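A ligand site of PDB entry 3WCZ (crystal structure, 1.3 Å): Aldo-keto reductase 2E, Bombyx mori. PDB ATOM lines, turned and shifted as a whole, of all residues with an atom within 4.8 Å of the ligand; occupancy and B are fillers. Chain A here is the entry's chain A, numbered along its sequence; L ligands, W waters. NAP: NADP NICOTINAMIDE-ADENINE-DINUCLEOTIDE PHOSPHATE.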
ATOM      1  N   GLY A  22      27.166   1.963 -29.458  1.00  0.00           N
ATOM      2  CA  GLY A  22      26.209   2.999 -29.800  1.00  0.00           C
ATOM      3  C   GLY A  22      26.747   3.996 -30.805  1.00  0.00           C
ATOM      4  O   GLY A  22      27.913   4.397 -30.727  1.00  0.00           O
ATOM      5  N   THR A  23      25.892   4.372 -31.751  1.00  0.00           N
ATOM      6  CA  THR A  23      26.257   5.358 -32.774  1.00  0.00           C
ATOM      7  C   THR A  23      25.299   6.515 -32.824  1.00  0.00           C
ATOM      8  O   THR A  23      25.316   7.295 -33.791  1.00  0.00           O
ATOM      9  CB  THR A  23      26.404   4.710 -34.163  1.00  0.00           C
ATOM     10  OG1 THR A  23      25.137   4.258 -34.657  1.00  0.00           O
ATOM     11  CG2 THR A  23      27.406   3.539 -34.153  1.00  0.00           C
ATOM     12  N   GLY A  24      24.486   6.699 -31.795  1.00  0.00           N
ATOM     13  CA  GLY A  24      23.727   7.924 -31.678  1.00  0.00           C
ATOM     14  C   GLY A  24      24.668   9.067 -31.362  1.00  0.00           C
ATOM     15  O   GLY A  24      25.766   8.882 -30.783  1.00  0.00           O
ATOM     16  N   THR A  27      25.591  12.774 -27.586  1.00  0.00           N
ATOM     17  CA  THR A  27      26.690  13.252 -26.751  1.00  0.00           C
ATOM     18  C   THR A  27      27.818  13.876 -27.565  1.00  0.00           C
ATOM     19  O   THR A  27      28.837  14.269 -26.986  1.00  0.00           O
ATOM     20  CB  THR A  27      27.270  12.112 -25.898  1.00  0.00           C
ATOM     21  OG1 THR A  27      27.894  11.132 -26.730  1.00  0.00           O
ATOM     22  CG2 THR A  27      26.186  11.476 -25.031  1.00  0.00           C
ATOM     23  N   LYS A  29      30.299  16.245 -29.266  1.00  0.00           N
ATOM     24  CA  LYS A  29      30.675  17.612 -28.907  1.00  0.00           C
ATOM     25  C   LYS A  29      30.775  18.433 -30.197  1.00  0.00           C
ATOM     26  O   LYS A  29      30.677  17.887 -31.294  1.00  0.00           O
ATOM     27  CB  LYS A  29      31.994  17.625 -28.136  1.00  0.00           C
ATOM     28  CG  LYS A  29      32.269  16.346 -27.327  1.00  0.00           C
ATOM     29  CD  LYS A  29      33.559  16.422 -26.504  1.00  0.00           C
ATOM     30  CE  LYS A  29      34.292  15.062 -26.447  1.00  0.00           C
ATOM     31  NZ  LYS A  29      33.453  13.861 -26.043  1.00  0.00           N
ATOM     32  N   ASP A  53      24.807  -0.686 -32.978  1.00  0.00           N
ATOM     33  CA  ASP A  53      23.453  -0.117 -32.889  1.00  0.00           C
ATOM     34  C   ASP A  53      23.435   1.232 -33.591  1.00  0.00           C
ATOM     35  O   ASP A  53      24.229   2.117 -33.240  1.00  0.00           O
ATOM     36  CB  ASP A  53      23.008   0.079 -31.424  1.00  0.00           C
ATOM     37  CG  ASP A  53      21.620   0.638 -31.322  1.00  0.00           C
ATOM     38  OD1 ASP A  53      20.670  -0.164 -31.446  1.00  0.00           O
ATOM     39  OD2 ASP A  53      21.449   1.864 -31.136  1.00  0.00           O
ATOM     40  N   TYR A  58      19.609   8.888 -36.880  1.00  0.00           N
ATOM     41  CA  TYR A  58      20.922   9.385 -36.519  1.00  0.00           C
ATOM     42  C   TYR A  58      21.662  10.004 -37.686  1.00  0.00           C
ATOM     43  O   TYR A  58      22.649  10.702 -37.484  1.00  0.00           O
ATOM     44  CB  TYR A  58      21.809   8.293 -35.896  1.00  0.00           C
ATOM     45  CG  TYR A  58      21.230   7.573 -34.714  1.00  0.00           C
ATOM     46  CD1 TYR A  58      20.206   8.108 -33.983  1.00  0.00           C
ATOM     47  CD2 TYR A  58      21.778   6.361 -34.286  1.00  0.00           C
ATOM     48  CE1 TYR A  58      19.677   7.434 -32.885  1.00  0.00           C
ATOM     49  CE2 TYR A  58      21.260   5.672 -33.200  1.00  0.00           C
ATOM     50  CZ  TYR A  58      20.216   6.202 -32.506  1.00  0.00           C
ATOM     51  OH  TYR A  58      19.683   5.507 -31.436  1.00  0.00           O
ATOM     52  N   LYS A  87      16.948   1.059 -37.008  1.00  0.00           N
ATOM     53  CA  LYS A  87      15.631   1.427 -36.482  1.00  0.00           C
ATOM     54  C   LYS A  87      14.835   2.222 -37.498  1.00  0.00           C
ATOM     55  O   LYS A  87      15.358   3.105 -38.201  1.00  0.00           O
ATOM     56  CB  LYS A  87      15.766   2.249 -35.180  1.00  0.00           C
ATOM     57  CG  LYS A  87      16.810   1.723 -34.200  1.00  0.00           C
ATOM     58  CD  LYS A  87      16.735   2.400 -32.850  1.00  0.00           C
ATOM     59  CE  LYS A  87      17.853   2.007 -31.927  1.00  0.00           C
ATOM     60  NZ  LYS A  87      19.135   2.657 -32.256  1.00  0.00           N
ATOM     61  N   HIS A 120      11.456   2.393 -33.736  1.00  0.00           N
ATOM     62  CA  HIS A 120      12.242   3.271 -32.853  1.00  0.00           C
ATOM     63  C   HIS A 120      11.412   3.808 -31.676  1.00  0.00           C
ATOM     64  O   HIS A 120      11.900   3.882 -30.561  1.00  0.00           O
ATOM     65  CB  HIS A 120      12.835   4.422 -33.697  1.00  0.00           C
ATOM     66  CG  HIS A 120      14.041   5.072 -33.095  1.00  0.00           C
ATOM     67  ND1 HIS A 120      15.069   5.570 -33.868  1.00  0.00           N
ATOM     68  CD2 HIS A 120      14.371   5.333 -31.806  1.00  0.00           C
ATOM     69  CE1 HIS A 120      15.987   6.103 -33.068  1.00  0.00           C
ATOM     70  NE2 HIS A 120      15.589   5.956 -31.813  1.00  0.00           N
ATOM     71  N   PHE A 121      10.165   4.190 -31.955  1.00  0.00           N
ATOM     72  CA  PHE A 121       9.192   4.580 -30.931  1.00  0.00           C
ATOM     73  C   PHE A 121       7.805   4.072 -31.338  1.00  0.00           C
ATOM     74  O   PHE A 121       7.525   3.902 -32.542  1.00  0.00           O
ATOM     75  CB  PHE A 121       9.067   6.115 -30.804  1.00  0.00           C
ATOM     76  CG  PHE A 121      10.235   6.778 -30.142  1.00  0.00           C
ATOM     77  CD1 PHE A 121      11.293   7.204 -30.917  1.00  0.00           C
ATOM     78  CD2 PHE A 121      10.247   7.032 -28.790  1.00  0.00           C
ATOM     79  CE1 PHE A 121      12.390   7.835 -30.322  1.00  0.00           C
ATOM     80  CE2 PHE A 121      11.344   7.621 -28.164  1.00  0.00           C
ATOM     81  CZ  PHE A 121      12.415   8.044 -28.938  1.00  0.00           C
ATOM     82  N   SER A 158      11.433  -0.494 -29.653  1.00  0.00           N
ATOM     83  CA  SER A 158      12.196   0.359 -28.756  1.00  0.00           C
ATOM     84  C   SER A 158      11.227   1.365 -28.148  1.00  0.00           C
ATOM     85  O   SER A 158      10.265   1.800 -28.820  1.00  0.00           O
ATOM     86  CB  SER A 158      13.287   1.057 -29.576  1.00  0.00           C
ATOM     87  OG  SER A 158      14.149   1.846 -28.776  1.00  0.00           O
ATOM     88  N   ASN A 159      11.468   1.736 -26.905  1.00  0.00           N
ATOM     89  CA  ASN A 159      10.646   2.731 -26.222  1.00  0.00           C
ATOM     90  C   ASN A 159       9.184   2.309 -26.113  1.00  0.00           C
ATOM     91  O   ASN A 159       8.285   3.146 -26.075  1.00  0.00           O
ATOM     92  CB  ASN A 159      10.759   4.104 -26.896  1.00  0.00           C
ATOM     93  CG  ASN A 159      12.159   4.621 -26.892  1.00  0.00           C
ATOM     94  OD1 ASN A 159      12.850   4.714 -27.941  1.00  0.00           O
ATOM     95  ND2 ASN A 159      12.604   4.980 -25.741  1.00  0.00           N
ATOM     96  N   GLN A 180      14.232  -2.182 -26.767  1.00  0.00           N
ATOM     97  CA  GLN A 180      15.375  -1.330 -26.461  1.00  0.00           C
ATOM     98  C   GLN A 180      14.895  -0.093 -25.715  1.00  0.00           C
ATOM     99  O   GLN A 180      14.119   0.706 -26.248  1.00  0.00           O
ATOM    100  CB  GLN A 180      16.138  -0.961 -27.744  1.00  0.00           C
ATOM    101  CG  GLN A 180      17.296   0.000 -27.491  1.00  0.00           C
ATOM    102  CD  GLN A 180      18.186   0.375 -28.666  1.00  0.00           C
ATOM    103  OE1 GLN A 180      18.510   1.558 -28.820  1.00  0.00           O
ATOM    104  NE2 GLN A 180      18.583  -0.588 -29.479  1.00  0.00           N
ATOM    105  N   TYR A 206      19.806   1.379 -23.532  1.00  0.00           N
ATOM    106  CA  TYR A 206      20.398   2.578 -24.087  1.00  0.00           C
ATOM    107  C   TYR A 206      20.728   3.619 -23.015  1.00  0.00           C
ATOM    108  O   TYR A 206      20.273   3.518 -21.886  1.00  0.00           O
ATOM    109  CB  TYR A 206      19.552   3.125 -25.239  1.00  0.00           C
ATOM    110  CG  TYR A 206      18.269   3.853 -24.974  1.00  0.00           C
ATOM    111  CD1 TYR A 206      18.228   5.091 -24.340  1.00  0.00           C
ATOM    112  CD2 TYR A 206      17.083   3.345 -25.481  1.00  0.00           C
ATOM    113  CE1 TYR A 206      17.038   5.799 -24.209  1.00  0.00           C
ATOM    114  CE2 TYR A 206      15.893   4.033 -25.342  1.00  0.00           C
ATOM    115  CZ  TYR A 206      15.884   5.271 -24.734  1.00  0.00           C
ATOM    116  OH  TYR A 206      14.740   6.007 -24.609  1.00  0.00           O
ATOM    117  N   SER A 207      21.551   4.594 -23.418  1.00  0.00           N
ATOM    118  CA  SER A 207      22.150   5.591 -22.524  1.00  0.00           C
ATOM    119  C   SER A 207      22.606   4.947 -21.218  1.00  0.00           C
ATOM    120  O   SER A 207      22.249   5.380 -20.139  1.00  0.00           O
ATOM    121  CB  SER A 207      21.164   6.742 -22.263  1.00  0.00           C
ATOM    122  OG  SER A 207      20.777   7.420 -23.460  1.00  0.00           O
ATOM    123  N   PRO A 208      23.416   3.894 -21.339  1.00  0.00           N
ATOM    124  CA  PRO A 208      23.795   3.103 -20.173  1.00  0.00           C
ATOM    125  C   PRO A 208      24.622   3.867 -19.127  1.00  0.00           C
ATOM    126  O   PRO A 208      24.642   3.435 -17.966  1.00  0.00           O
ATOM    127  CB  PRO A 208      24.635   1.969 -20.771  1.00  0.00           C
ATOM    128  CG  PRO A 208      25.221   2.550 -22.004  1.00  0.00           C
ATOM    129  CD  PRO A 208      24.089   3.414 -22.557  1.00  0.00           C
ATOM    130  N   PHE A 209      25.294   4.962 -19.509  1.00  0.00           N
ATOM    131  CA  PHE A 209      26.077   5.706 -18.536  1.00  0.00           C
ATOM    132  C   PHE A 209      25.235   6.729 -17.777  1.00  0.00           C
ATOM    133  O   PHE A 209      25.743   7.368 -16.826  1.00  0.00           O
ATOM    134  CB  PHE A 209      27.283   6.361 -19.197  1.00  0.00           C
ATOM    135  CG  PHE A 209      28.265   5.362 -19.762  1.00  0.00           C
ATOM    136  CD1 PHE A 209      28.880   4.430 -18.930  1.00  0.00           C
ATOM    137  CD2 PHE A 209      28.549   5.333 -21.096  1.00  0.00           C
ATOM    138  CE1 PHE A 209      29.791   3.526 -19.468  1.00  0.00           C
ATOM    139  CE2 PHE A 209      29.467   4.479 -21.615  1.00  0.00           C
ATOM    140  CZ  PHE A 209      30.083   3.567 -20.819  1.00  0.00           C
ATOM    141  N   GLY A 210      23.966   6.898 -18.127  1.00  0.00           N
ATOM    142  CA  GLY A 210      23.090   7.764 -17.350  1.00  0.00           C
ATOM    143  C   GLY A 210      23.662   9.171 -17.262  1.00  0.00           C
ATOM    144  O   GLY A 210      24.233   9.679 -18.209  1.00  0.00           O
ATOM    145  N   VAL A 213      28.037  10.507 -16.919  1.00  0.00           N
ATOM    146  CA  VAL A 213      28.766  11.247 -17.957  1.00  0.00           C
ATOM    147  C   VAL A 213      28.001  12.539 -18.240  1.00  0.00           C
ATOM    148  O   VAL A 213      26.806  12.656 -17.950  1.00  0.00           O
ATOM    149  CB  VAL A 213      28.910  10.434 -19.275  1.00  0.00           C
ATOM    150  CG1 VAL A 213      29.694   9.198 -19.021  1.00  0.00           C
ATOM    151  CG2 VAL A 213      27.519  10.101 -19.903  1.00  0.00           C
ATOM    152  N   ARG A 215      25.786  15.362 -19.806  1.00  0.00           N
ATOM    153  CA  ARG A 215      24.662  15.444 -20.716  1.00  0.00           C
ATOM    154  C   ARG A 215      24.369  16.893 -21.130  1.00  0.00           C
ATOM    155  O   ARG A 215      23.287  17.201 -21.614  1.00  0.00           O
ATOM    156  CB  ARG A 215      23.409  14.823 -20.088  1.00  0.00           C
ATOM    157  CG  ARG A 215      23.604  13.349 -19.745  1.00  0.00           C
ATOM    158  CD  ARG A 215      23.820  12.526 -20.994  1.00  0.00           C
ATOM    159  NE  ARG A 215      24.003  11.120 -20.625  1.00  0.00           N
ATOM    160  CZ  ARG A 215      24.025  10.103 -21.483  1.00  0.00           C
ATOM    161  NH1 ARG A 215      23.900  10.323 -22.777  1.00  0.00           N
ATOM    162  NH2 ARG A 215      24.169   8.856 -21.031  1.00  0.00           N
ATOM    163  N   SER A 240      37.171   0.214 -14.350  1.00  0.00           N
ATOM    164  CA  SER A 240      36.802   1.602 -14.319  1.00  0.00           C
ATOM    165  C   SER A 240      35.348   1.759 -13.886  1.00  0.00           C
ATOM    166  O   SER A 240      34.596   0.805 -13.919  1.00  0.00           O
ATOM    167  CB  SER A 240      36.977   2.231 -15.688  1.00  0.00           C
ATOM    168  OG  SER A 240      35.987   1.708 -16.571  1.00  0.00           O
ATOM    169  N   GLY A 242      33.106   3.261 -15.563  1.00  0.00           N
ATOM    170  CA  GLY A 242      32.317   2.953 -16.746  1.00  0.00           C
ATOM    171  C   GLY A 242      32.080   1.455 -16.842  1.00  0.00           C
ATOM    172  O   GLY A 242      30.989   1.005 -17.204  1.00  0.00           O
ATOM    173  N   ILE A 257      24.369  -0.642 -24.562  1.00  0.00           N
ATOM    174  CA  ILE A 257      24.774  -0.006 -25.816  1.00  0.00           C
ATOM    175  C   ILE A 257      25.702   1.181 -25.546  1.00  0.00           C
ATOM    176  O   ILE A 257      25.339   2.342 -25.796  1.00  0.00           O
ATOM    177  CB  ILE A 257      23.552   0.494 -26.615  1.00  0.00           C
ATOM    178  CG1 ILE A 257      22.404  -0.517 -26.624  1.00  0.00           C
ATOM    179  CG2 ILE A 257      23.962   0.831 -28.048  1.00  0.00           C
ATOM    180  CD1 ILE A 257      21.131   0.066 -27.217  1.00  0.00           C
ATOM    181  N   PRO A 258      26.905   0.932 -25.042  1.00  0.00           N
ATOM    182  CA  PRO A 258      27.795   2.068 -24.766  1.00  0.00           C
ATOM    183  C   PRO A 258      28.224   2.779 -26.049  1.00  0.00           C
ATOM    184  O   PRO A 258      28.768   2.146 -26.972  1.00  0.00           O
ATOM    185  CB  PRO A 258      28.998   1.404 -24.067  1.00  0.00           C
ATOM    186  CG  PRO A 258      29.004   0.033 -24.584  1.00  0.00           C
ATOM    187  CD  PRO A 258      27.551  -0.344 -24.697  1.00  0.00           C
ATOM    188  N   LYS A 259      28.018   4.094 -26.104  1.00  0.00           N
ATOM    189  CA  LYS A 259      28.539   4.917 -27.188  1.00  0.00           C
ATOM    190  C   LYS A 259      29.932   5.444 -26.795  1.00  0.00           C
ATOM    191  O   LYS A 259      30.153   5.974 -25.709  1.00  0.00           O
ATOM    192  CB  LYS A 259      27.626   6.108 -27.491  1.00  0.00           C
ATOM    193  CG  LYS A 259      28.210   7.112 -28.493  1.00  0.00           C
ATOM    194  CD  LYS A 259      29.036   8.213 -27.829  1.00  0.00           C
ATOM    195  CE  LYS A 259      29.563   9.203 -28.827  1.00  0.00           C
ATOM    196  NZ  LYS A 259      30.393  10.273 -28.133  1.00  0.00           N
ATOM    197  N   SER A 260      30.878   5.285 -27.717  1.00  0.00           N
ATOM    198  CA  SER A 260      32.151   5.978 -27.594  1.00  0.00           C
ATOM    199  C   SER A 260      32.697   6.192 -28.970  1.00  0.00           C
ATOM    200  O   SER A 260      32.454   5.410 -29.884  1.00  0.00           O
ATOM    201  CB  SER A 260      33.145   5.171 -26.769  1.00  0.00           C
ATOM    202  OG  SER A 260      34.385   5.865 -26.607  1.00  0.00           O
ATOM    203  N   THR A 261      33.453   7.287 -29.106  1.00  0.00           N
ATOM    204  CA  THR A 261      34.250   7.502 -30.280  1.00  0.00           C
ATOM    205  C   THR A 261      35.749   7.557 -29.924  1.00  0.00           C
ATOM    206  O   THR A 261      36.560   7.984 -30.759  1.00  0.00           O
ATOM    207  CB  THR A 261      33.841   8.770 -31.034  1.00  0.00           C
ATOM    208  OG1 THR A 261      33.842   9.875 -30.136  1.00  0.00           O
ATOM    209  CG2 THR A 261      32.459   8.591 -31.646  1.00  0.00           C
ATOM    210  N   ASN A 262      36.097   7.089 -28.739  1.00  0.00           N
ATOM    211  CA  ASN A 262      37.486   7.085 -28.254  1.00  0.00           C
ATOM    212  C   ASN A 262      38.028   5.656 -28.278  1.00  0.00           C
ATOM    213  O   ASN A 262      37.404   4.770 -27.717  1.00  0.00           O
ATOM    214  CB  ASN A 262      37.518   7.628 -26.813  1.00  0.00           C
ATOM    215  CG  ASN A 262      38.895   7.538 -26.126  1.00  0.00           C
ATOM    216  OD1 ASN A 262      39.253   6.554 -25.529  1.00  0.00           O
ATOM    217  ND2 ASN A 262      39.648   8.636 -26.219  1.00  0.00           N
ATOM    218  N   ARG A 265      38.407   3.952 -24.755  1.00  0.00           N
ATOM    219  CA  ARG A 265      37.147   3.701 -24.037  1.00  0.00           C
ATOM    220  C   ARG A 265      36.306   2.655 -24.768  1.00  0.00           C
ATOM    221  O   ARG A 265      35.674   1.836 -24.131  1.00  0.00           O
ATOM    222  CB  ARG A 265      36.368   4.966 -23.788  1.00  0.00           C
ATOM    223  CG  ARG A 265      37.084   5.847 -22.768  1.00  0.00           C
ATOM    224  CD  ARG A 265      36.214   6.996 -22.393  1.00  0.00           C
ATOM    225  NE  ARG A 265      36.181   8.073 -23.369  1.00  0.00           N
ATOM    226  CZ  ARG A 265      37.062   9.058 -23.448  1.00  0.00           C
ATOM    227  NH1 ARG A 265      38.115   9.079 -22.654  1.00  0.00           N
ATOM    228  NH2 ARG A 265      36.889  10.012 -24.351  1.00  0.00           N
ATOM    229  N   GLN A 268      37.660  -0.530 -23.522  1.00  0.00           N
ATOM    230  CA  GLN A 268      37.277  -0.762 -22.127  1.00  0.00           C
ATOM    231  C   GLN A 268      35.839  -1.222 -21.993  1.00  0.00           C
ATOM    232  O   GLN A 268      35.505  -2.055 -21.159  1.00  0.00           O
ATOM    233  CB  GLN A 268      37.464   0.515 -21.330  1.00  0.00           C
ATOM    234  CG  GLN A 268      38.924   0.860 -21.152  1.00  0.00           C
ATOM    235  CD  GLN A 268      39.146   2.075 -20.293  1.00  0.00           C
ATOM    236  OE1 GLN A 268      38.411   3.059 -20.356  1.00  0.00           O
ATOM    237  NE2 GLN A 268      40.184   2.007 -19.453  1.00  0.00           N
ATOM    238  N   ASN A 269      34.978  -0.697 -22.861  1.00  0.00           N
ATOM    239  CA  ASN A 269      33.543  -0.865 -22.690  1.00  0.00           C
ATOM    240  C   ASN A 269      33.043  -2.278 -23.049  1.00  0.00           C
ATOM    241  O   ASN A 269      31.914  -2.619 -22.722  1.00  0.00           O
ATOM    242  CB  ASN A 269      32.792   0.182 -23.516  1.00  0.00           C
ATOM    243  CG  ASN A 269      32.875   1.569 -22.936  1.00  0.00           C
ATOM    244  OD1 ASN A 269      33.290   1.760 -21.773  1.00  0.00           O
ATOM    245  ND2 ASN A 269      32.521   2.570 -23.718  1.00  0.00           N
ATOM    246  N   ILE A 295      16.886  10.638 -21.880  1.00  0.00           N
ATOM    247  CA  ILE A 295      16.213  10.941 -23.152  1.00  0.00           C
ATOM    248  C   ILE A 295      14.790  11.410 -22.857  1.00  0.00           C
ATOM    249  O   ILE A 295      13.921  10.647 -22.473  1.00  0.00           O
ATOM    250  CB  ILE A 295      16.246   9.710 -24.120  1.00  0.00           C
ATOM    251  CG1 ILE A 295      17.700   9.294 -24.415  1.00  0.00           C
ATOM    252  CG2 ILE A 295      15.472   9.991 -25.405  1.00  0.00           C
ATOM    253  CD1 ILE A 295      18.562  10.346 -25.108  1.00  0.00           C
HETATM  254  PA  NAP L   1      26.054   6.688 -23.480  1.00  0.00           P
HETATM  255  O1A NAP L   1      26.663   5.498 -24.084  1.00  0.00           O
HETATM  256  O2A NAP L   1      25.060   6.624 -22.424  1.00  0.00           O
HETATM  257  O5B NAP L   1      27.099   7.780 -23.077  1.00  0.00           O
HETATM  258  C5B NAP L   1      28.091   8.182 -23.962  1.00  0.00           C
HETATM  259  C4B NAP L   1      29.077   9.181 -23.362  1.00  0.00           C
HETATM  260  O4B NAP L   1      29.915   8.508 -22.404  1.00  0.00           O
HETATM  261  C3B NAP L   1      29.984   9.869 -24.321  1.00  0.00           C
HETATM  262  O3B NAP L   1      30.131  11.192 -23.862  1.00  0.00           O
HETATM  263  C2B NAP L   1      31.212   9.102 -24.219  1.00  0.00           C
HETATM  264  O2B NAP L   1      32.375   9.818 -24.581  1.00  0.00           O
HETATM  265  C1B NAP L   1      31.255   8.700 -22.767  1.00  0.00           C
HETATM  266  N9A NAP L   1      31.938   7.465 -22.442  1.00  0.00           N
HETATM  267  C8A NAP L   1      31.872   6.321 -23.151  1.00  0.00           C
HETATM  268  N7A NAP L   1      32.507   5.347 -22.543  1.00  0.00           N
HETATM  269  C5A NAP L   1      33.032   5.849 -21.385  1.00  0.00           C
HETATM  270  C6A NAP L   1      33.799   5.304 -20.353  1.00  0.00           C
HETATM  271  N6A NAP L   1      34.241   3.979 -20.324  1.00  0.00           N
HETATM  272  N1A NAP L   1      34.137   6.131 -19.349  1.00  0.00           N
HETATM  273  C2A NAP L   1      33.735   7.403 -19.344  1.00  0.00           C
HETATM  274  N3A NAP L   1      32.997   7.961 -20.319  1.00  0.00           N
HETATM  275  C4A NAP L   1      32.634   7.173 -21.333  1.00  0.00           C
HETATM  276  O3  NAP L   1      25.401   7.508 -24.715  1.00  0.00           O
HETATM  277  PN  NAP L   1      24.042   7.569 -25.541  1.00  0.00           P
HETATM  278  O1N NAP L   1      24.451   7.939 -26.925  1.00  0.00           O
HETATM  279  O2N NAP L   1      23.088   8.437 -24.805  1.00  0.00           O
HETATM  280  O5D NAP L   1      23.415   6.107 -25.530  1.00  0.00           O
HETATM  281  C5D NAP L   1      24.093   5.033 -26.099  1.00  0.00           C
HETATM  282  C4D NAP L   1      23.500   4.486 -27.394  1.00  0.00           C
HETATM  283  O4D NAP L   1      22.205   3.953 -27.198  1.00  0.00           O
HETATM  284  C3D NAP L   1      23.295   5.509 -28.465  1.00  0.00           C
HETATM  285  O3D NAP L   1      24.503   5.946 -29.046  1.00  0.00           O
HETATM  286  C2D NAP L   1      22.388   4.814 -29.364  1.00  0.00           C
HETATM  287  O2D NAP L   1      23.054   3.834 -30.086  1.00  0.00           O
HETATM  288  C1D NAP L   1      21.421   4.208 -28.376  1.00  0.00           C
HETATM  289  N1N NAP L   1      20.225   4.965 -27.979  1.00  0.00           N
HETATM  290  C2N NAP L   1      19.008   4.593 -28.429  1.00  0.00           C
HETATM  291  C3N NAP L   1      17.902   5.302 -28.052  1.00  0.00           C
HETATM  292  C7N NAP L   1      16.591   4.800 -28.547  1.00  0.00           C
HETATM  293  O7N NAP L   1      16.425   3.610 -28.906  1.00  0.00           O
HETATM  294  N7N NAP L   1      15.551   5.650 -28.454  1.00  0.00           N
HETATM  295  C4N NAP L   1      18.002   6.458 -27.263  1.00  0.00           C
HETATM  296  C5N NAP L   1      19.270   6.836 -26.788  1.00  0.00           C
HETATM  297  C6N NAP L   1      20.346   6.053 -27.171  1.00  0.00           C
HETATM  298  P2B NAP L   1      33.401   9.285 -25.695  1.00  0.00           P
HETATM  299  O1X NAP L   1      34.434  10.423 -25.799  1.00  0.00           O
HETATM  300  O2X NAP L   1      34.035   8.059 -25.182  1.00  0.00           O
HETATM  301  O3X NAP L   1      32.609   9.092 -26.968  1.00  0.00           O
HETATM  302  O   HOH W   1      34.992   5.196 -16.649  1.00  0.00           O
HETATM  303  O   HOH W   2      22.183  10.762 -26.197  1.00  0.00           O
HETATM  304  O   HOH W   3      30.851  12.536 -26.188  1.00  0.00           O
HETATM  305  O   HOH W   4      25.908   9.865 -28.147  1.00  0.00           O
HETATM  306  O   HOH W   5      33.091  10.862 -20.191  1.00  0.00           O
HETATM  307  O   HOH W   6      29.528  13.177 -22.106  1.00  0.00           O
HETATM  308  O   HOH W   7      16.231   8.269 -29.850  1.00  0.00           O
HETATM  309  O   HOH W   8      35.612  10.738 -28.200  1.00  0.00           O
HETATM  310  O   HOH W   9      22.811   9.485 -28.733  1.00  0.00           O
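The side-chain hydroxyl of Ser 260 sits at hydrogen-bond distance from an oxygen (O2X) of the ligand, at 2.6 Å.
OD2 of Asp 53 sits at hydrogen-bond distance from O2D of the ligand (2.7 Å).
The backbone NH (N) of Lys 259 is in hydrogen-bond range of an oxygen (O1A) of the ligand (2.8 Å).
The side-chain amino group (NZ) of Lys 259 is in salt-bridge range of an oxygen (O3X) of the ligand (2.8 Å).
The guanidinium group (NH2) of Arg 215 is in salt-bridge range of an oxygen (O2A) of the ligand, 2.8 Å away.
The guanidinium group (NE) of Arg 265 lies within salt-bridge range of an oxygen (O2X) of the ligand.
OD1 of Asn 269 sits at hydrogen-bond distance from N6A of the ligand (2.8 Å).
The backbone NH of Gly 24 sits at hydrogen-bond distance from an oxygen (O3D) of the ligand, at 2.9 Å.
The backbone NH (N) of Ser 207 sits at hydrogen-bond distance from an oxygen (O5D) of the ligand, at 3.2 Å.
The side-chain hydroxyl (OG) of Ser 207 sits at hydrogen-bond distance from an oxygen (O2N) of the ligand (2.9 Å).
O7N of the ligand lies within hydrogen-bond range of OG of Ser 158, at 2.9 Å.
N7N of the ligand sits at hydrogen-bond distance from OD1 of Asn 159 (2.9 Å).
The backbone NH (N) of Thr 261 sits at hydrogen-bond distance from an oxygen (O3X) of the ligand (2.9 Å).
The side-chain hydroxyl (OG1) of Thr 261 sits at hydrogen-bond distance from an oxygen (O3X) of the ligand, 3.5 Å away.
An oxygen (O7N) of the ligand lies close to the side-chain amide oxygen (OE1) of Gln 180.
The backbone NH (N) of Phe 209 lies within hydrogen-bond range of an oxygen (O2A) of the ligand, at 3.4 Å.
The backbone NH (N) of Thr 23 sits at hydrogen-bond distance from an oxygen (O2D) of the ligand (3.3 Å).
N7N of the ligand is in hydrogen-bond range of NE2 of His 120.
NZ of Lys 29 is in salt-bridge range of O1X of the ligand (3.6 Å).
The backbone NH of Asn 262 sits at hydrogen-bond distance from the side-chain hydroxyl of Ser 260, at 3.0 Å.
The side-chain carboxylate of Asp 53 is in hydrogen-bond range of the side-chain amide nitrogen of Gln 180.
The side-chain hydroxyl (OG1) of Thr 23 lies within hydrogen-bond range of the backbone carbonyl oxygen (O) of Asp 53, 2.7 Å away.
NZ of Lys 87 is in salt-bridge range of OD2 of Asp 53, 2.7 Å away.
The backbone NH (N) of Arg 265 lies within hydrogen-bond range of the side-chain amide oxygen (OD1) of Asn 262 (2.8 Å).
OD1 of Asn 159 lies within hydrogen-bond range of OG of Ser 158.
OG of Ser 158 lies within hydrogen-bond range of O of Gln 180 (2.8 Å).
The side-chain amide oxygen (OD1) of Asn 159 sits close to the backbone carbonyl oxygen (O) of His 120 (2.9 Å).
An oxygen (O2A) of the ligand lies close to the backbone nitrogen (N) of Pro 208 (3.4 Å).
Merely in contact with the ligand: Gly 22 (3.3 Å), Thr 27 (3.4 Å), Tyr 58 (3.2 Å), Lys 87 (3.7 Å), Phe 121 (3.97 Å), Tyr 206 (3.2 Å), Val 213 (3.5 Å), Ile 257 (3.0 Å), Pro 258 (3.7 Å), Asn 262 (3.9 Å) and Ile 295 (3.8 Å).
Hydrophobic or aromatic side chains that line the ligand: His 120, Phe 121, Tyr 206, Pro 208, Phe 209, Val 213, Ile 257 and Ile 295.
Of the 32 residues printed, 28 come within 4 Å of the ligand.
Along chain A the residues within 4 Å of the ligand span positions 22 to 295.
The nearest printed residue that does not touch the ligand is Gly 242 (4.2 Å).
Water W8 bridges an oxygen (O1X) of the ligand (2.7 Å) and the side-chain hydroxyl (OG1) of Thr 261 (2.8 Å).
Water W4 lies within hydrogen-bond range of an oxygen (O1N) of the ligand (2.7 Å), the side-chain hydroxyl (OG1) of Thr 27 (2.7 Å) and the backbone carbonyl oxygen (O) of Gly 24 (2.8 Å).
Water W3 lies within hydrogen-bond range of O of Thr 27, O3B of the ligand, NZ of Lys 29 and NZ of Lys 259.
Water W1 lies within hydrogen-bond range of N of Gly 242 (2.9 Å) and N1A of the ligand (3.0 Å).
Water W7 lies within hydrogen-bond range of a nitrogen (N7N) of the ligand and a ring nitrogen (NE2) of His 120.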
